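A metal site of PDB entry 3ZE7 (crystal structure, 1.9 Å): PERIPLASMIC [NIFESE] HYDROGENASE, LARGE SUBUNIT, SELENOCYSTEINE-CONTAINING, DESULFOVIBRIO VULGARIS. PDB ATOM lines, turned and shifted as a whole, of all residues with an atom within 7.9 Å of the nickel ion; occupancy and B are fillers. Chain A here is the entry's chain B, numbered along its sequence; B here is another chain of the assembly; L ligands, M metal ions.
Four residues have an atom within 4 Å of the nickel ion: OCS 64, Cys 67, SEC 478 and Cys 481. The nearest printed residue that does not touch the nickel ion is Arg 411 (4.6 Å).
OD1 of OCS 64 sits at hydrogen-bond distance from N of Val 66 (2.5 Å). N of SEC 478 is in hydrogen-bond range of the side-chain hydroxyl (OG) of Ser 434 (2.9 Å). The side-chain sulfur (SG) of Cys 481 lies close to a ring nitrogen (NE2) of His 71, at 3.2 Å. O of Cys 481 sits at hydrogen-bond distance from OG of Ser 432 (2.6 Å).
FE1 of LIG L1 is bound by SG of Cys 67, 2.3 Å away. An iron atom (FE1) of LIG L1 is bound by the side-chain sulfur of Cys 481, at 2.3 Å. The backbone NH of Arg 411 sits at hydrogen-bond distance from a nitrogen (N2) of LIG L1. N2 of LIG L1 sits at hydrogen-bond distance from NH1 of Arg 411 (3.2 Å). A nitrogen (N1) of LIG L1 sits at hydrogen-bond distance from the backbone NH (N) of Ser 434 (2.9 Å). OG of Ser 434 is in hydrogen-bond range of N1 of LIG L1, at 2.8 Å. O of Cys 67 sits close to S1 of LG2 L2, 3.7 Å away. The backbone NH of Ala 70 sits close to a sulfur (S1) of LG2 L2.
The nickel ion is bound by SG of OCS 64 (2.2 Å). SE of SEC 478 binds the nickel ion. SG of Cys 67 is bound to the nickel ion (2.3 Å). SG of Cys 481 binds the nickel ion, at 2.5 Å.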
ATOM      1  N   GLU A  17      30.960  26.250  18.042  1.00  0.00           N
ATOM      2  CA  GLU A  17      30.322  25.014  18.511  1.00  0.00           C
ATOM      3  C   GLU A  17      31.344  23.887  18.405  1.00  0.00           C
ATOM      4  O   GLU A  17      32.006  23.759  17.374  1.00  0.00           O
ATOM      5  CB  GLU A  17      29.062  24.662  17.686  1.00  0.00           C
ATOM      6  CG  GLU A  17      28.169  23.544  18.317  1.00  0.00           C
ATOM      7  CD  GLU A  17      28.792  22.148  18.253  1.00  0.00           C
ATOM      8  OE1 GLU A  17      29.489  21.830  17.260  1.00  0.00           O
ATOM      9  OE2 GLU A  17      28.588  21.349  19.201  1.00  0.00           O
ATOM     10  N   ARG A  42      31.596  10.932  17.283  1.00  0.00           N
ATOM     11  CA  ARG A  42      30.471  10.113  17.771  1.00  0.00           C
ATOM     12  C   ARG A  42      30.081   8.953  16.835  1.00  0.00           C
ATOM     13  O   ARG A  42      29.735   7.858  17.322  1.00  0.00           O
ATOM     14  CB  ARG A  42      29.252  11.003  18.078  1.00  0.00           C
ATOM     15  CG  ARG A  42      29.443  11.835  19.338  1.00  0.00           C
ATOM     16  CD  ARG A  42      28.436  12.959  19.428  1.00  0.00           C
ATOM     17  NE  ARG A  42      28.629  13.902  18.334  1.00  0.00           N
ATOM     18  CZ  ARG A  42      27.727  14.804  17.967  1.00  0.00           C
ATOM     19  NH1 ARG A  42      26.578  14.897  18.602  1.00  0.00           N
ATOM     20  NH2 ARG A  42      27.981  15.611  16.935  1.00  0.00           N
ATOM     21  N   GLN A  61      19.324  14.825  14.134  1.00  0.00           N
ATOM     22  CA  GLN A  61      19.311  16.159  14.700  1.00  0.00           C
ATOM     23  C   GLN A  61      20.269  16.281  15.875  1.00  0.00           C
ATOM     24  O   GLN A  61      20.766  17.373  16.175  1.00  0.00           O
ATOM     25  CB  GLN A  61      17.906  16.552  15.159  1.00  0.00           C
ATOM     26  CG  GLN A  61      16.978  16.902  14.018  1.00  0.00           C
ATOM     27  CD  GLN A  61      15.678  17.440  14.523  1.00  0.00           C
ATOM     28  OE1 GLN A  61      15.562  18.631  14.805  1.00  0.00           O
ATOM     29  NE2 GLN A  61      14.688  16.559  14.655  1.00  0.00           N
ATOM     30  N   ILE A  63      23.139  15.343  15.967  1.00  0.00           N
ATOM     31  CA  ILE A  63      24.464  15.741  15.507  1.00  0.00           C
ATOM     32  C   ILE A  63      24.807  17.132  16.068  1.00  0.00           C
ATOM     33  O   ILE A  63      25.952  17.398  16.425  1.00  0.00           O
ATOM     34  CB  ILE A  63      24.574  15.705  13.951  1.00  0.00           C
ATOM     35  CG1 ILE A  63      24.660  14.249  13.470  1.00  0.00           C
ATOM     36  CG2 ILE A  63      25.779  16.528  13.448  1.00  0.00           C
ATOM     37  CD1 ILE A  63      24.466  14.075  11.981  1.00  0.00           C
ATOM     38  N   OCS A  64      23.808  18.001  16.197  1.00  0.00           N
ATOM     39  CA  OCS A  64      24.087  19.395  16.517  1.00  0.00           C
ATOM     40  CB  OCS A  64      24.566  20.103  15.235  1.00  0.00           C
ATOM     41  SG  OCS A  64      25.372  21.536  15.601  1.00  0.00           S
ATOM     42  C   OCS A  64      22.829  20.085  17.051  1.00  0.00           C
ATOM     43  O   OCS A  64      21.726  20.134  16.177  1.00  0.00           O
ATOM     44  OD1 OCS A  64      24.470  22.370  16.337  1.00  0.00           O
ATOM     45  OD2 OCS A  64      26.501  21.208  16.428  1.00  0.00           O
ATOM     46  N   GLY A  65      22.834  20.642  18.258  1.00  0.00           N
ATOM     47  CA  GLY A  65      21.650  21.261  18.791  1.00  0.00           C
ATOM     48  C   GLY A  65      21.590  22.754  18.520  1.00  0.00           C
ATOM     49  O   GLY A  65      20.674  23.433  18.989  1.00  0.00           O
ATOM     50  N   VAL A  66      22.583  23.257  17.788  1.00  0.00           N
ATOM     51  CA  VAL A  66      22.527  24.621  17.271  1.00  0.00           C
ATOM     52  C   VAL A  66      21.880  24.619  15.892  1.00  0.00           C
ATOM     53  O   VAL A  66      21.020  25.455  15.600  1.00  0.00           O
ATOM     54  CB  VAL A  66      23.923  25.273  17.178  1.00  0.00           C
ATOM     55  CG1 VAL A  66      23.788  26.711  16.671  1.00  0.00           C
ATOM     56  CG2 VAL A  66      24.627  25.232  18.527  1.00  0.00           C
ATOM     57  N   CYS A  67      22.257  23.671  15.046  1.00  0.00           N
ATOM     58  CA  CYS A  67      21.649  23.562  13.732  1.00  0.00           C
ATOM     59  C   CYS A  67      20.824  22.269  13.478  1.00  0.00           C
ATOM     60  O   CYS A  67      20.947  21.661  12.419  1.00  0.00           O
ATOM     61  CB  CYS A  67      22.730  23.659  12.649  1.00  0.00           C
ATOM     62  SG  CYS A  67      23.885  22.217  12.620  1.00  0.00           S
ATOM     63  N   PRO A  68      19.956  21.848  14.422  1.00  0.00           N
ATOM     64  CA  PRO A  68      19.282  20.564  14.168  1.00  0.00           C
ATOM     65  C   PRO A  68      18.268  20.607  13.035  1.00  0.00           C
ATOM     66  O   PRO A  68      18.120  19.601  12.343  1.00  0.00           O
ATOM     67  CB  PRO A  68      18.568  20.267  15.492  1.00  0.00           C
ATOM     68  CG  PRO A  68      18.337  21.625  16.098  1.00  0.00           C
ATOM     69  CD  PRO A  68      19.523  22.458  15.698  1.00  0.00           C
ATOM     70  N   ALA A  70      18.536  21.957  10.279  1.00  0.00           N
ATOM     71  CA  ALA A  70      19.264  21.682   9.044  1.00  0.00           C
ATOM     72  C   ALA A  70      19.373  20.169   8.740  1.00  0.00           C
ATOM     73  O   ALA A  70      19.094  19.719   7.612  1.00  0.00           O
ATOM     74  CB  ALA A  70      20.660  22.331   9.088  1.00  0.00           C
ATOM     75  N   HIS A  71      19.769  19.396   9.733  1.00  0.00           N
ATOM     76  CA  HIS A  71      19.888  17.953   9.544  1.00  0.00           C
ATOM     77  C   HIS A  71      18.522  17.313   9.406  1.00  0.00           C
ATOM     78  O   HIS A  71      18.353  16.372   8.647  1.00  0.00           O
ATOM     79  CB  HIS A  71      20.675  17.315  10.700  1.00  0.00           C
ATOM     80  CG  HIS A  71      22.122  17.657  10.694  1.00  0.00           C
ATOM     81  ND1 HIS A  71      23.024  17.054   9.840  1.00  0.00           N
ATOM     82  CD2 HIS A  71      22.827  18.555  11.419  1.00  0.00           C
ATOM     83  CE1 HIS A  71      24.217  17.561  10.049  1.00  0.00           C
ATOM     84  NE2 HIS A  71      24.129  18.473  11.000  1.00  0.00           N
ATOM     85  N   SER A 106      20.293  31.212  14.606  1.00  0.00           N
ATOM     86  CA  SER A 106      21.682  30.780  14.507  1.00  0.00           C
ATOM     87  C   SER A 106      22.623  31.922  14.136  1.00  0.00           C
ATOM     88  O   SER A 106      23.693  32.027  14.703  1.00  0.00           O
ATOM     89  CB  SER A 106      21.802  29.621  13.523  1.00  0.00           C
ATOM     90  OG  SER A 106      23.138  29.172  13.443  1.00  0.00           O
ATOM     91  N   ALA A 409      22.495  24.460   5.512  1.00  0.00           N
ATOM     92  CA  ALA A 409      22.531  24.792   6.926  1.00  0.00           C
ATOM     93  C   ALA A 409      22.978  26.246   7.052  1.00  0.00           C
ATOM     94  O   ALA A 409      23.604  26.789   6.126  1.00  0.00           O
ATOM     95  CB  ALA A 409      23.530  23.885   7.628  1.00  0.00           C
ATOM     96  N   PRO A 410      22.663  26.894   8.190  1.00  0.00           N
ATOM     97  CA  PRO A 410      23.146  28.267   8.439  1.00  0.00           C
ATOM     98  C   PRO A 410      24.646  28.437   8.233  1.00  0.00           C
ATOM     99  O   PRO A 410      25.097  29.511   7.852  1.00  0.00           O
ATOM    100  CB  PRO A 410      22.801  28.469   9.909  1.00  0.00           C
ATOM    101  CG  PRO A 410      21.521  27.636  10.103  1.00  0.00           C
ATOM    102  CD  PRO A 410      21.722  26.435   9.222  1.00  0.00           C
ATOM    103  N   ARG A 411      25.414  27.376   8.468  1.00  0.00           N
ATOM    104  CA  ARG A 411      26.862  27.421   8.276  1.00  0.00           C
ATOM    105  C   ARG A 411      27.349  26.976   6.905  1.00  0.00           C
ATOM    106  O   ARG A 411      28.535  27.115   6.586  1.00  0.00           O
ATOM    107  CB  ARG A 411      27.546  26.611   9.374  1.00  0.00           C
ATOM    108  CG  ARG A 411      27.382  27.260  10.708  1.00  0.00           C
ATOM    109  CD  ARG A 411      27.574  26.345  11.911  1.00  0.00           C
ATOM    110  NE  ARG A 411      27.369  27.198  13.075  1.00  0.00           N
ATOM    111  CZ  ARG A 411      26.178  27.564  13.515  1.00  0.00           C
ATOM    112  NH1 ARG A 411      25.073  27.077  12.960  1.00  0.00           N
ATOM    113  NH2 ARG A 411      26.086  28.409  14.546  1.00  0.00           N
ATOM    114  N   SER A 432      28.579  17.620   5.658  1.00  0.00           N
ATOM    115  CA  SER A 432      28.028  18.801   6.328  1.00  0.00           C
ATOM    116  C   SER A 432      28.779  20.099   6.063  1.00  0.00           C
ATOM    117  O   SER A 432      29.847  20.107   5.450  1.00  0.00           O
ATOM    118  CB  SER A 432      27.993  18.549   7.836  1.00  0.00           C
ATOM    119  OG  SER A 432      29.316  18.320   8.295  1.00  0.00           O
ATOM    120  N   ALA A 433      28.199  21.199   6.535  1.00  0.00           N
ATOM    121  CA  ALA A 433      28.733  22.531   6.285  1.00  0.00           C
ATOM    122  C   ALA A 433      30.143  22.725   6.807  1.00  0.00           C
ATOM    123  O   ALA A 433      31.053  23.025   6.037  1.00  0.00           O
ATOM    124  CB  ALA A 433      27.805  23.566   6.882  1.00  0.00           C
ATOM    125  N   SER A 434      30.346  22.553   8.119  1.00  0.00           N
ATOM    126  CA  SER A 434      31.666  22.796   8.701  1.00  0.00           C
ATOM    127  C   SER A 434      32.683  21.716   8.315  1.00  0.00           C
ATOM    128  O   SER A 434      33.894  21.902   8.489  1.00  0.00           O
ATOM    129  CB  SER A 434      31.578  22.968  10.216  1.00  0.00           C
ATOM    130  OG  SER A 434      30.941  24.193  10.529  1.00  0.00           O
ATOM    131  N   ASP A 476      32.042  30.716  11.547  1.00  0.00           N
ATOM    132  CA  ASP A 476      30.994  30.096  12.379  1.00  0.00           C
ATOM    133  C   ASP A 476      31.182  28.564  12.465  1.00  0.00           C
ATOM    134  O   ASP A 476      30.266  27.806  12.140  1.00  0.00           O
ATOM    135  CB  ASP A 476      29.618  30.514  11.820  1.00  0.00           C
ATOM    136  CG  ASP A 476      28.460  30.166  12.736  1.00  0.00           C
ATOM    137  OD1 ASP A 476      28.684  29.715  13.885  1.00  0.00           O
ATOM    138  OD2 ASP A 476      27.298  30.370  12.293  1.00  0.00           O
ATOM    139  N   PRO A 477      32.381  28.114  12.899  1.00  0.00           N
ATOM    140  CA  PRO A 477      32.655  26.669  12.851  1.00  0.00           C
ATOM    141  C   PRO A 477      31.751  25.860  13.775  1.00  0.00           C
ATOM    142  O   PRO A 477      31.393  26.321  14.862  1.00  0.00           O
ATOM    143  CB  PRO A 477      34.094  26.550  13.373  1.00  0.00           C
ATOM    144  CG  PRO A 477      34.611  27.930  13.519  1.00  0.00           C
ATOM    145  CD  PRO A 477      33.460  28.859  13.578  1.00  0.00           C
ATOM    146  N   SEC A 478      31.413  24.648  13.343  1.00  0.00           N
ATOM    147  CA  SEC A 478      30.579  23.749  14.134  1.00  0.00           C
ATOM    148  CB  SEC A 478      29.148  23.847  13.611  1.00  0.00           C
ATOM    149 SE   SEC A 478      27.992  22.640  14.648  1.00  0.00          SE
ATOM    150  C   SEC A 478      31.162  22.362  13.994  1.00  0.00           C
ATOM    151  O   SEC A 478      30.950  21.671  12.992  1.00  0.00           O
ATOM    152  N   LEU A 479      31.956  21.969  14.985  1.00  0.00           N
ATOM    153  CA  LEU A 479      32.723  20.740  14.872  1.00  0.00           C
ATOM    154  C   LEU A 479      31.896  19.483  15.149  1.00  0.00           C
ATOM    155  O   LEU A 479      32.250  18.395  14.719  1.00  0.00           O
ATOM    156  CB  LEU A 479      33.987  20.802  15.758  1.00  0.00           C
ATOM    157  CG  LEU A 479      35.224  21.430  15.089  1.00  0.00           C
ATOM    158  CD1 LEU A 479      35.676  20.583  13.907  1.00  0.00           C
ATOM    159  CD2 LEU A 479      34.970  22.865  14.626  1.00  0.00           C
ATOM    160  N   GLY A 480      30.786  19.644  15.877  1.00  0.00           N
ATOM    161  CA  GLY A 480      29.809  18.589  16.021  1.00  0.00           C
ATOM    162  C   GLY A 480      29.294  18.176  14.661  1.00  0.00           C
ATOM    163  O   GLY A 480      29.247  16.981  14.327  1.00  0.00           O
ATOM    164  N   CYS A 481      28.913  19.174  13.864  1.00  0.00           N
ATOM    165  CA  CYS A 481      28.527  18.946  12.478  1.00  0.00           C
ATOM    166  C   CYS A 481      29.663  18.436  11.603  1.00  0.00           C
ATOM    167  O   CYS A 481      29.452  17.562  10.770  1.00  0.00           O
ATOM    168  CB  CYS A 481      27.974  20.237  11.847  1.00  0.00           C
ATOM    169  SG  CYS A 481      26.255  20.491  12.186  1.00  0.00           S
ATOM    170  N   ALA A 482      30.861  18.975  11.779  1.00  0.00           N
ATOM    171  CA  ALA A 482      31.968  18.623  10.892  1.00  0.00           C
ATOM    172  C   ALA A 482      32.325  17.126  10.998  1.00  0.00           C
ATOM    173  O   ALA A 482      32.649  16.479   9.999  1.00  0.00           O
ATOM    174  CB  ALA A 482      33.214  19.500  11.169  1.00  0.00           C
ATOM    175  N   CYS B  18      26.104  17.705  21.686  1.00  0.00           N
ATOM    176  CA  CYS B  18      25.741  18.390  20.442  1.00  0.00           C
ATOM    177  C   CYS B  18      25.493  19.875  20.678  1.00  0.00           C
ATOM    178  O   CYS B  18      25.015  20.583  19.767  1.00  0.00           O
ATOM    179  CB  CYS B  18      24.485  17.763  19.832  1.00  0.00           C
ATOM    180  SG  CYS B  18      22.947  18.208  20.696  1.00  0.00           S
ATOM    181  N   THR B  19      25.804  20.337  21.883  1.00  0.00           N
ATOM    182  CA  THR B  19      25.552  21.725  22.300  1.00  0.00           C
ATOM    183  C   THR B  19      24.047  22.068  22.477  1.00  0.00           C
ATOM    184  O   THR B  19      23.666  23.171  22.857  1.00  0.00           O
ATOM    185  CB  THR B  19      26.358  22.745  21.421  1.00  0.00           C
ATOM    186  OG1 THR B  19      27.713  22.308  21.378  1.00  0.00           O
ATOM    187  CG2 THR B  19      26.333  24.166  21.984  1.00  0.00           C
HETATM  188 FE1  LIG L   1      25.644  22.531  11.215  1.00  0.00          FE
HETATM  189  C1  LIG L   1      27.313  22.887  10.600  1.00  0.00           C
HETATM  190  N1  LIG L   1      28.364  23.174  10.174  1.00  0.00           N
HETATM  191  C2  LIG L   1      25.056  24.205  10.761  1.00  0.00           C
HETATM  192  N2  LIG L   1      24.682  25.244  10.406  1.00  0.00           N
HETATM  193  C3  LIG L   1      25.177  21.672   9.685  1.00  0.00           C
HETATM  194  O1  LIG L   1      25.031  21.246   8.647  1.00  0.00           O
HETATM  195  S1  LG2 L   2      19.450  24.855  11.314  1.00  0.00           S
HETATM  196 NI    NI M   1      25.936  22.458  13.707  1.00  0.00          NI
